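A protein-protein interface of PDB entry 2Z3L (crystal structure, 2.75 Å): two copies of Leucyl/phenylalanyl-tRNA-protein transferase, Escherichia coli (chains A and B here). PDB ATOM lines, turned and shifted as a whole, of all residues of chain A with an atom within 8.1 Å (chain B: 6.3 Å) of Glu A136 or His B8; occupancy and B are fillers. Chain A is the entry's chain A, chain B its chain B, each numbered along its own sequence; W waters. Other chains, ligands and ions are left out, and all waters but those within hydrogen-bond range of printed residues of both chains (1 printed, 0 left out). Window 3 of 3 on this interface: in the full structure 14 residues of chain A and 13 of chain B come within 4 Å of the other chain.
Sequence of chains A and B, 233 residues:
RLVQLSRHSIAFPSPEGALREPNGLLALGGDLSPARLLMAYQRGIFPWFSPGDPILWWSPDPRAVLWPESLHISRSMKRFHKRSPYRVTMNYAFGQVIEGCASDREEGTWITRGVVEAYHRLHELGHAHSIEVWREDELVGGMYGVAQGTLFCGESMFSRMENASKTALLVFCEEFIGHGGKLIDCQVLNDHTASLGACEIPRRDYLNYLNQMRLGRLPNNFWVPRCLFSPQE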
ATOM      1  N   PRO A  85     -25.459 -20.848  21.805  1.00  0.00           N
ATOM      2  CA  PRO A  85     -25.658 -21.403  23.143  1.00  0.00           C
ATOM      3  C   PRO A  85     -25.289 -22.889  23.097  1.00  0.00           C
ATOM      4  O   PRO A  85     -25.455 -23.621  24.069  1.00  0.00           O
ATOM      5  CB  PRO A  85     -27.147 -21.194  23.360  1.00  0.00           C
ATOM      6  CG  PRO A  85     -27.697 -21.551  22.009  1.00  0.00           C
ATOM      7  CD  PRO A  85     -26.720 -20.901  21.036  1.00  0.00           C
ATOM      8  N   TYR A  86     -24.787 -23.318  21.946  1.00  0.00           N
ATOM      9  CA  TYR A  86     -24.416 -24.707  21.730  1.00  0.00           C
ATOM     10  C   TYR A  86     -22.918 -24.970  21.726  1.00  0.00           C
ATOM     11  O   TYR A  86     -22.102 -24.076  21.487  1.00  0.00           O
ATOM     12  CB  TYR A  86     -24.989 -25.182  20.398  1.00  0.00           C
ATOM     13  CG  TYR A  86     -26.487 -25.097  20.329  1.00  0.00           C
ATOM     14  CD1 TYR A  86     -27.122 -24.633  19.173  1.00  0.00           C
ATOM     15  CD2 TYR A  86     -27.287 -25.506  21.415  1.00  0.00           C
ATOM     16  CE1 TYR A  86     -28.512 -24.579  19.096  1.00  0.00           C
ATOM     17  CE2 TYR A  86     -28.691 -25.458  21.346  1.00  0.00           C
ATOM     18  CZ  TYR A  86     -29.291 -24.991  20.181  1.00  0.00           C
ATOM     19  OH  TYR A  86     -30.661 -24.929  20.084  1.00  0.00           O
ATOM     20  N   ARG A  87     -22.570 -26.220  21.986  1.00  0.00           N
ATOM     21  CA  ARG A  87     -21.190 -26.653  21.968  1.00  0.00           C
ATOM     22  C   ARG A  87     -21.201 -27.792  20.926  1.00  0.00           C
ATOM     23  O   ARG A  87     -22.156 -28.569  20.877  1.00  0.00           O
ATOM     24  CB  ARG A  87     -20.808 -27.138  23.372  1.00  0.00           C
ATOM     25  CG  ARG A  87     -19.337 -27.470  23.598  1.00  0.00           C
ATOM     26  CD  ARG A  87     -19.015 -27.467  25.104  1.00  0.00           C
ATOM     27  NE  ARG A  87     -18.450 -26.190  25.559  1.00  0.00           N
ATOM     28  CZ  ARG A  87     -18.724 -25.611  26.729  1.00  0.00           C
ATOM     29  NH1 ARG A  87     -19.570 -26.188  27.577  1.00  0.00           N
ATOM     30  NH2 ARG A  87     -18.145 -24.460  27.058  1.00  0.00           N
ATOM     31  N   VAL A 133     -24.219 -31.906  18.947  1.00  0.00           N
ATOM     32  CA  VAL A 133     -24.541 -30.535  19.309  1.00  0.00           C
ATOM     33  C   VAL A 133     -25.077 -30.589  20.735  1.00  0.00           C
ATOM     34  O   VAL A 133     -26.103 -31.219  20.998  1.00  0.00           O
ATOM     35  CB  VAL A 133     -25.611 -29.934  18.389  1.00  0.00           C
ATOM     36  CG1 VAL A 133     -25.948 -28.508  18.837  1.00  0.00           C
ATOM     37  CG2 VAL A 133     -25.108 -29.923  16.969  1.00  0.00           C
ATOM     38  N   TRP A 134     -24.369 -29.935  21.653  1.00  0.00           N
ATOM     39  CA  TRP A 134     -24.742 -29.918  23.066  1.00  0.00           C
ATOM     40  C   TRP A 134     -25.230 -28.564  23.549  1.00  0.00           C
ATOM     41  O   TRP A 134     -24.670 -27.525  23.192  1.00  0.00           O
ATOM     42  CB  TRP A 134     -23.547 -30.304  23.954  1.00  0.00           C
ATOM     43  CG  TRP A 134     -22.893 -31.579  23.587  1.00  0.00           C
ATOM     44  CD1 TRP A 134     -21.931 -31.773  22.627  1.00  0.00           C
ATOM     45  CD2 TRP A 134     -23.187 -32.866  24.127  1.00  0.00           C
ATOM     46  NE1 TRP A 134     -21.613 -33.111  22.538  1.00  0.00           N
ATOM     47  CE2 TRP A 134     -22.371 -33.803  23.448  1.00  0.00           C
ATOM     48  CE3 TRP A 134     -24.065 -33.325  25.120  1.00  0.00           C
ATOM     49  CZ2 TRP A 134     -22.413 -35.168  23.731  1.00  0.00           C
ATOM     50  CZ3 TRP A 134     -24.106 -34.678  25.402  1.00  0.00           C
ATOM     51  CH2 TRP A 134     -23.285 -35.586  24.710  1.00  0.00           C
ATOM     52  N   ARG A 135     -26.274 -28.587  24.369  1.00  0.00           N
ATOM     53  CA  ARG A 135     -26.802 -27.380  24.975  1.00  0.00           C
ATOM     54  C   ARG A 135     -26.524 -27.656  26.436  1.00  0.00           C
ATOM     55  O   ARG A 135     -27.309 -28.330  27.097  1.00  0.00           O
ATOM     56  CB  ARG A 135     -28.309 -27.251  24.737  1.00  0.00           C
ATOM     57  CG  ARG A 135     -28.953 -26.099  25.493  1.00  0.00           C
ATOM     58  CD  ARG A 135     -28.142 -24.807  25.363  1.00  0.00           C
ATOM     59  NE  ARG A 135     -28.629 -23.795  26.296  1.00  0.00           N
ATOM     60  CZ  ARG A 135     -27.895 -22.808  26.800  1.00  0.00           C
ATOM     61  NH1 ARG A 135     -26.615 -22.669  26.466  1.00  0.00           N
ATOM     62  NH2 ARG A 135     -28.446 -21.966  27.661  1.00  0.00           N
ATOM     63  N   GLU A 136     -25.400 -27.151  26.941  1.00  0.00           N
ATOM     64  CA  GLU A 136     -25.013 -27.420  28.325  1.00  0.00           C
ATOM     65  C   GLU A 136     -24.642 -28.917  28.398  1.00  0.00           C
ATOM     66  O   GLU A 136     -23.810 -29.398  27.626  1.00  0.00           O
ATOM     67  CB  GLU A 136     -26.174 -27.114  29.293  1.00  0.00           C
ATOM     68  CG  GLU A 136     -26.557 -25.633  29.426  1.00  0.00           C
ATOM     69  CD  GLU A 136     -27.743 -25.404  30.378  1.00  0.00           C
ATOM     70  OE1 GLU A 136     -27.807 -26.095  31.417  1.00  0.00           O
ATOM     71  OE2 GLU A 136     -28.603 -24.530  30.101  1.00  0.00           O
ATOM     72  N   ASP A 137     -25.286 -29.652  29.302  1.00  0.00           N
ATOM     73  CA  ASP A 137     -25.028 -31.086  29.482  1.00  0.00           C
ATOM     74  C   ASP A 137     -26.030 -31.990  28.750  1.00  0.00           C
ATOM     75  O   ASP A 137     -26.070 -33.198  28.996  1.00  0.00           O
ATOM     76  CB  ASP A 137     -25.063 -31.430  30.974  1.00  0.00           C
ATOM     77  CG  ASP A 137     -26.476 -31.375  31.561  1.00  0.00           C
ATOM     78  OD1 ASP A 137     -27.246 -30.439  31.236  1.00  0.00           O
ATOM     79  OD2 ASP A 137     -26.811 -32.271  32.366  1.00  0.00           O
ATOM     80  N   GLU A 138     -26.827 -31.405  27.854  1.00  0.00           N
ATOM     81  CA  GLU A 138     -27.844 -32.147  27.106  1.00  0.00           C
ATOM     82  C   GLU A 138     -27.591 -32.222  25.604  1.00  0.00           C
ATOM     83  O   GLU A 138     -27.373 -31.205  24.951  1.00  0.00           O
ATOM     84  CB  GLU A 138     -29.215 -31.510  27.332  1.00  0.00           C
ATOM     85  CG  GLU A 138     -30.376 -32.304  26.766  1.00  0.00           C
ATOM     86  CD  GLU A 138     -30.709 -33.523  27.613  1.00  0.00           C
ATOM     87  OE1 GLU A 138     -29.801 -34.039  28.312  1.00  0.00           O
ATOM     88  OE2 GLU A 138     -31.878 -33.973  27.570  1.00  0.00           O
ATOM     89  N   LEU A 139     -27.618 -33.434  25.059  1.00  0.00           N
ATOM     90  CA  LEU A 139     -27.426 -33.616  23.623  1.00  0.00           C
ATOM     91  C   LEU A 139     -28.741 -33.121  23.014  1.00  0.00           C
ATOM     92  O   LEU A 139     -29.807 -33.665  23.307  1.00  0.00           O
ATOM     93  CB  LEU A 139     -27.191 -35.097  23.285  1.00  0.00           C
ATOM     94  CG  LEU A 139     -26.865 -35.421  21.817  1.00  0.00           C
ATOM     95  CD1 LEU A 139     -25.497 -34.848  21.445  1.00  0.00           C
ATOM     96  CD2 LEU A 139     -26.882 -36.929  21.593  1.00  0.00           C
ATOM     97  N   VAL A 140     -28.672 -32.084  22.187  1.00  0.00           N
ATOM     98  CA  VAL A 140     -29.881 -31.520  21.599  1.00  0.00           C
ATOM     99  C   VAL A 140     -29.935 -31.611  20.080  1.00  0.00           C
ATOM    100  O   VAL A 140     -30.880 -31.133  19.456  1.00  0.00           O
ATOM    101  CB  VAL A 140     -30.054 -30.040  22.033  1.00  0.00           C
ATOM    102  CG1 VAL A 140     -30.306 -29.970  23.531  1.00  0.00           C
ATOM    103  CG2 VAL A 140     -28.804 -29.239  21.684  1.00  0.00           C
ATOM    104  N   MET A 161     -33.612 -28.867  19.646  1.00  0.00           N
ATOM    105  CA  MET A 161     -33.582 -27.452  20.028  1.00  0.00           C
ATOM    106  C   MET A 161     -33.340 -26.578  18.796  1.00  0.00           C
ATOM    107  O   MET A 161     -32.517 -26.906  17.946  1.00  0.00           O
ATOM    108  CB  MET A 161     -32.487 -27.218  21.071  1.00  0.00           C
ATOM    109  CG  MET A 161     -32.794 -26.101  22.043  1.00  0.00           C
ATOM    110  SD  MET A 161     -31.852 -26.265  23.568  1.00  0.00           S
ATOM    111  CE  MET A 161     -31.782 -24.535  24.131  1.00  0.00           C
ATOM    112  N   PRO A 231     -19.252 -22.635  23.087  1.00  0.00           N
ATOM    113  CA  PRO A 231     -20.119 -21.460  23.239  1.00  0.00           C
ATOM    114  C   PRO A 231     -19.553 -20.371  24.158  1.00  0.00           C
ATOM    115  O   PRO A 231     -18.466 -20.526  24.736  1.00  0.00           O
ATOM    116  CB  PRO A 231     -21.409 -22.063  23.790  1.00  0.00           C
ATOM    117  CG  PRO A 231     -20.888 -23.159  24.680  1.00  0.00           C
ATOM    118  CD  PRO A 231     -19.811 -23.793  23.816  1.00  0.00           C
ATOM    119  N   SER B   6     -22.850 -26.893  38.192  1.00  0.00           N
ATOM    120  CA  SER B   6     -24.293 -26.940  37.963  1.00  0.00           C
ATOM    121  C   SER B   6     -24.542 -27.571  36.595  1.00  0.00           C
ATOM    122  O   SER B   6     -23.606 -27.766  35.818  1.00  0.00           O
ATOM    123  CB  SER B   6     -24.901 -25.532  37.999  1.00  0.00           C
ATOM    124  OG  SER B   6     -24.413 -24.715  36.953  1.00  0.00           O
ATOM    125  N   ARG B   7     -25.800 -27.890  36.301  1.00  0.00           N
ATOM    126  CA  ARG B   7     -26.141 -28.492  35.014  1.00  0.00           C
ATOM    127  C   ARG B   7     -26.054 -27.443  33.891  1.00  0.00           C
ATOM    128  O   ARG B   7     -25.974 -27.775  32.705  1.00  0.00           O
ATOM    129  CB  ARG B   7     -27.557 -29.066  35.066  1.00  0.00           C
ATOM    130  CG  ARG B   7     -28.627 -27.997  35.211  1.00  0.00           C
ATOM    131  CD  ARG B   7     -30.011 -28.523  34.842  1.00  0.00           C
ATOM    132  NE  ARG B   7     -30.884 -27.455  34.348  1.00  0.00           N
ATOM    133  CZ  ARG B   7     -31.285 -26.405  35.067  1.00  0.00           C
ATOM    134  NH1 ARG B   7     -30.899 -26.269  36.332  1.00  0.00           N
ATOM    135  NH2 ARG B   7     -32.067 -25.481  34.514  1.00  0.00           N
ATOM    136  N   HIS B   8     -26.056 -26.174  34.279  1.00  0.00           N
ATOM    137  CA  HIS B   8     -26.004 -25.087  33.317  1.00  0.00           C
ATOM    138  C   HIS B   8     -24.744 -25.068  32.483  1.00  0.00           C
ATOM    139  O   HIS B   8     -24.741 -24.577  31.356  1.00  0.00           O
ATOM    140  CB  HIS B   8     -26.179 -23.752  34.036  1.00  0.00           C
ATOM    141  CG  HIS B   8     -27.451 -23.663  34.816  1.00  0.00           C
ATOM    142  ND1 HIS B   8     -27.648 -24.351  35.994  1.00  0.00           N
ATOM    143  CD2 HIS B   8     -28.609 -23.011  34.562  1.00  0.00           C
ATOM    144  CE1 HIS B   8     -28.874 -24.126  36.432  1.00  0.00           C
ATOM    145  NE2 HIS B   8     -29.477 -23.317  35.580  1.00  0.00           N
ATOM    146  N   SER B   9     -23.665 -25.601  33.031  1.00  0.00           N
ATOM    147  CA  SER B   9     -22.423 -25.625  32.284  1.00  0.00           C
ATOM    148  C   SER B   9     -21.686 -26.938  32.460  1.00  0.00           C
ATOM    149  O   SER B   9     -21.645 -27.504  33.548  1.00  0.00           O
ATOM    150  CB  SER B   9     -21.522 -24.471  32.709  1.00  0.00           C
ATOM    151  OG  SER B   9     -20.283 -24.541  32.026  1.00  0.00           O
ATOM    152  N   ILE B  10     -21.109 -27.416  31.370  1.00  0.00           N
ATOM    153  CA  ILE B  10     -20.361 -28.654  31.379  1.00  0.00           C
ATOM    154  C   ILE B  10     -18.893 -28.251  31.446  1.00  0.00           C
ATOM    155  O   ILE B  10     -17.975 -29.078  31.347  1.00  0.00           O
ATOM    156  CB  ILE B  10     -20.707 -29.468  30.110  1.00  0.00           C
ATOM    157  CG1 ILE B  10     -21.124 -30.869  30.523  1.00  0.00           C
ATOM    158  CG2 ILE B  10     -19.560 -29.496  29.134  1.00  0.00           C
ATOM    159  CD1 ILE B  10     -22.179 -30.882  31.603  1.00  0.00           C
ATOM    160  N   ALA B  35     -20.961 -36.010  28.529  1.00  0.00           N
ATOM    161  CA  ALA B  35     -20.419 -34.727  28.103  1.00  0.00           C
ATOM    162  C   ALA B  35     -19.507 -34.106  29.145  1.00  0.00           C
ATOM    163  O   ALA B  35     -18.409 -33.640  28.831  1.00  0.00           O
ATOM    164  CB  ALA B  35     -21.560 -33.767  27.774  1.00  0.00           C
ATOM    165  N   ARG B  36     -19.970 -34.090  30.387  1.00  0.00           N
ATOM    166  CA  ARG B  36     -19.188 -33.504  31.458  1.00  0.00           C
ATOM    167  C   ARG B  36     -17.916 -34.312  31.727  1.00  0.00           C
ATOM    168  O   ARG B  36     -16.848 -33.739  31.972  1.00  0.00           O
ATOM    169  CB  ARG B  36     -20.043 -33.390  32.715  1.00  0.00           C
ATOM    170  CG  ARG B  36     -19.294 -32.915  33.928  1.00  0.00           C
ATOM    171  CD  ARG B  36     -20.274 -32.488  34.977  1.00  0.00           C
ATOM    172  NE  ARG B  36     -20.815 -31.175  34.658  1.00  0.00           N
ATOM    173  CZ  ARG B  36     -22.050 -30.787  34.950  1.00  0.00           C
ATOM    174  NH1 ARG B  36     -22.880 -31.617  35.562  1.00  0.00           N
ATOM    175  NH2 ARG B  36     -22.453 -29.565  34.641  1.00  0.00           N
HETATM  176  O   HOH W   1     -24.088 -36.052  28.815  1.00  0.00           O
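The side-chain carboxylate of Glu A136 lies close to the backbone NH of His B8, 3.4 Å away. The side-chain carboxylate (OE1) of Glu A136 sits close to the backbone carbonyl oxygen (O) of Arg B7, 2.8 Å away. OD1 of Asp A137 sits close to O of Arg B7.
O of Arg A87 is in hydrogen-bond range of N of Trp A134 (2.7 Å). NH2 of Arg A135 is in salt-bridge range of OE2 of Glu A136. The side-chain hydroxyl (OG) of Ser B6 lies within hydrogen-bond range of a ring nitrogen (ND1) of His B8 (3.4 Å). A ring nitrogen (NE2) of His B8 lies close to the guanidinium group (NH1) of Arg B7 (3.4 Å).
Among the printed residues, pairs that only touch across the chains: Arg A87 with Ile B10, Trp A134 with Ala B35, Glu A136 with Ile B10 and Asp A137 with Ile B10.
Of the printed residues of chain B, Arg A87 touches Ile B10 (3.7 Å). Of the printed residues of chain B, Trp A134 touches Ala B35 (3.6 Å). Glu A136 touches just these residues of chain B: Arg B7, His B8 and Ile B10. Glu A138 touches none of the printed residues of chain B. Printed residues of chain A within 4 Å of Arg B7: Glu A136 (2.8 Å) and Asp A137 (3.3 Å). Printed residues of chain A within 4 Å of Ile B10: Arg A87, Glu A136 and Asp A137. Of the printed residues of chain A, Ala B35 touches Trp A134 (3.6 Å). The nearest residue of chain B that does not touch Glu A136 is Ser B9 (4.5 Å). The nearest residue of chain A that does not touch His B8 is Asp A137 (5.4 Å).
Of the 7 printed residues of chain B, 4 touch a printed residue of chain A. Of the 13 printed residues of chain A, 4 touch a printed residue of chain B. Hydrophobic or aromatic side chains of chain A that line the printed part of chain B: Trp A134. Among the printed residues, 7 pairs touch across the chains. Among the printed residues, no Asp or Glu carboxylate lies within 4 Å of a Lys or Arg side-chain nitrogen of the other chain.
No position is printed for both chains. Of the 7 pairs that touch across the chains among the printed residues, none has its exchanged pair printed and touching as well.
Water W1 lies within hydrogen-bond range of N of Ala B35 (3.1 Å) and O of Asp A137 (3.5 Å).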
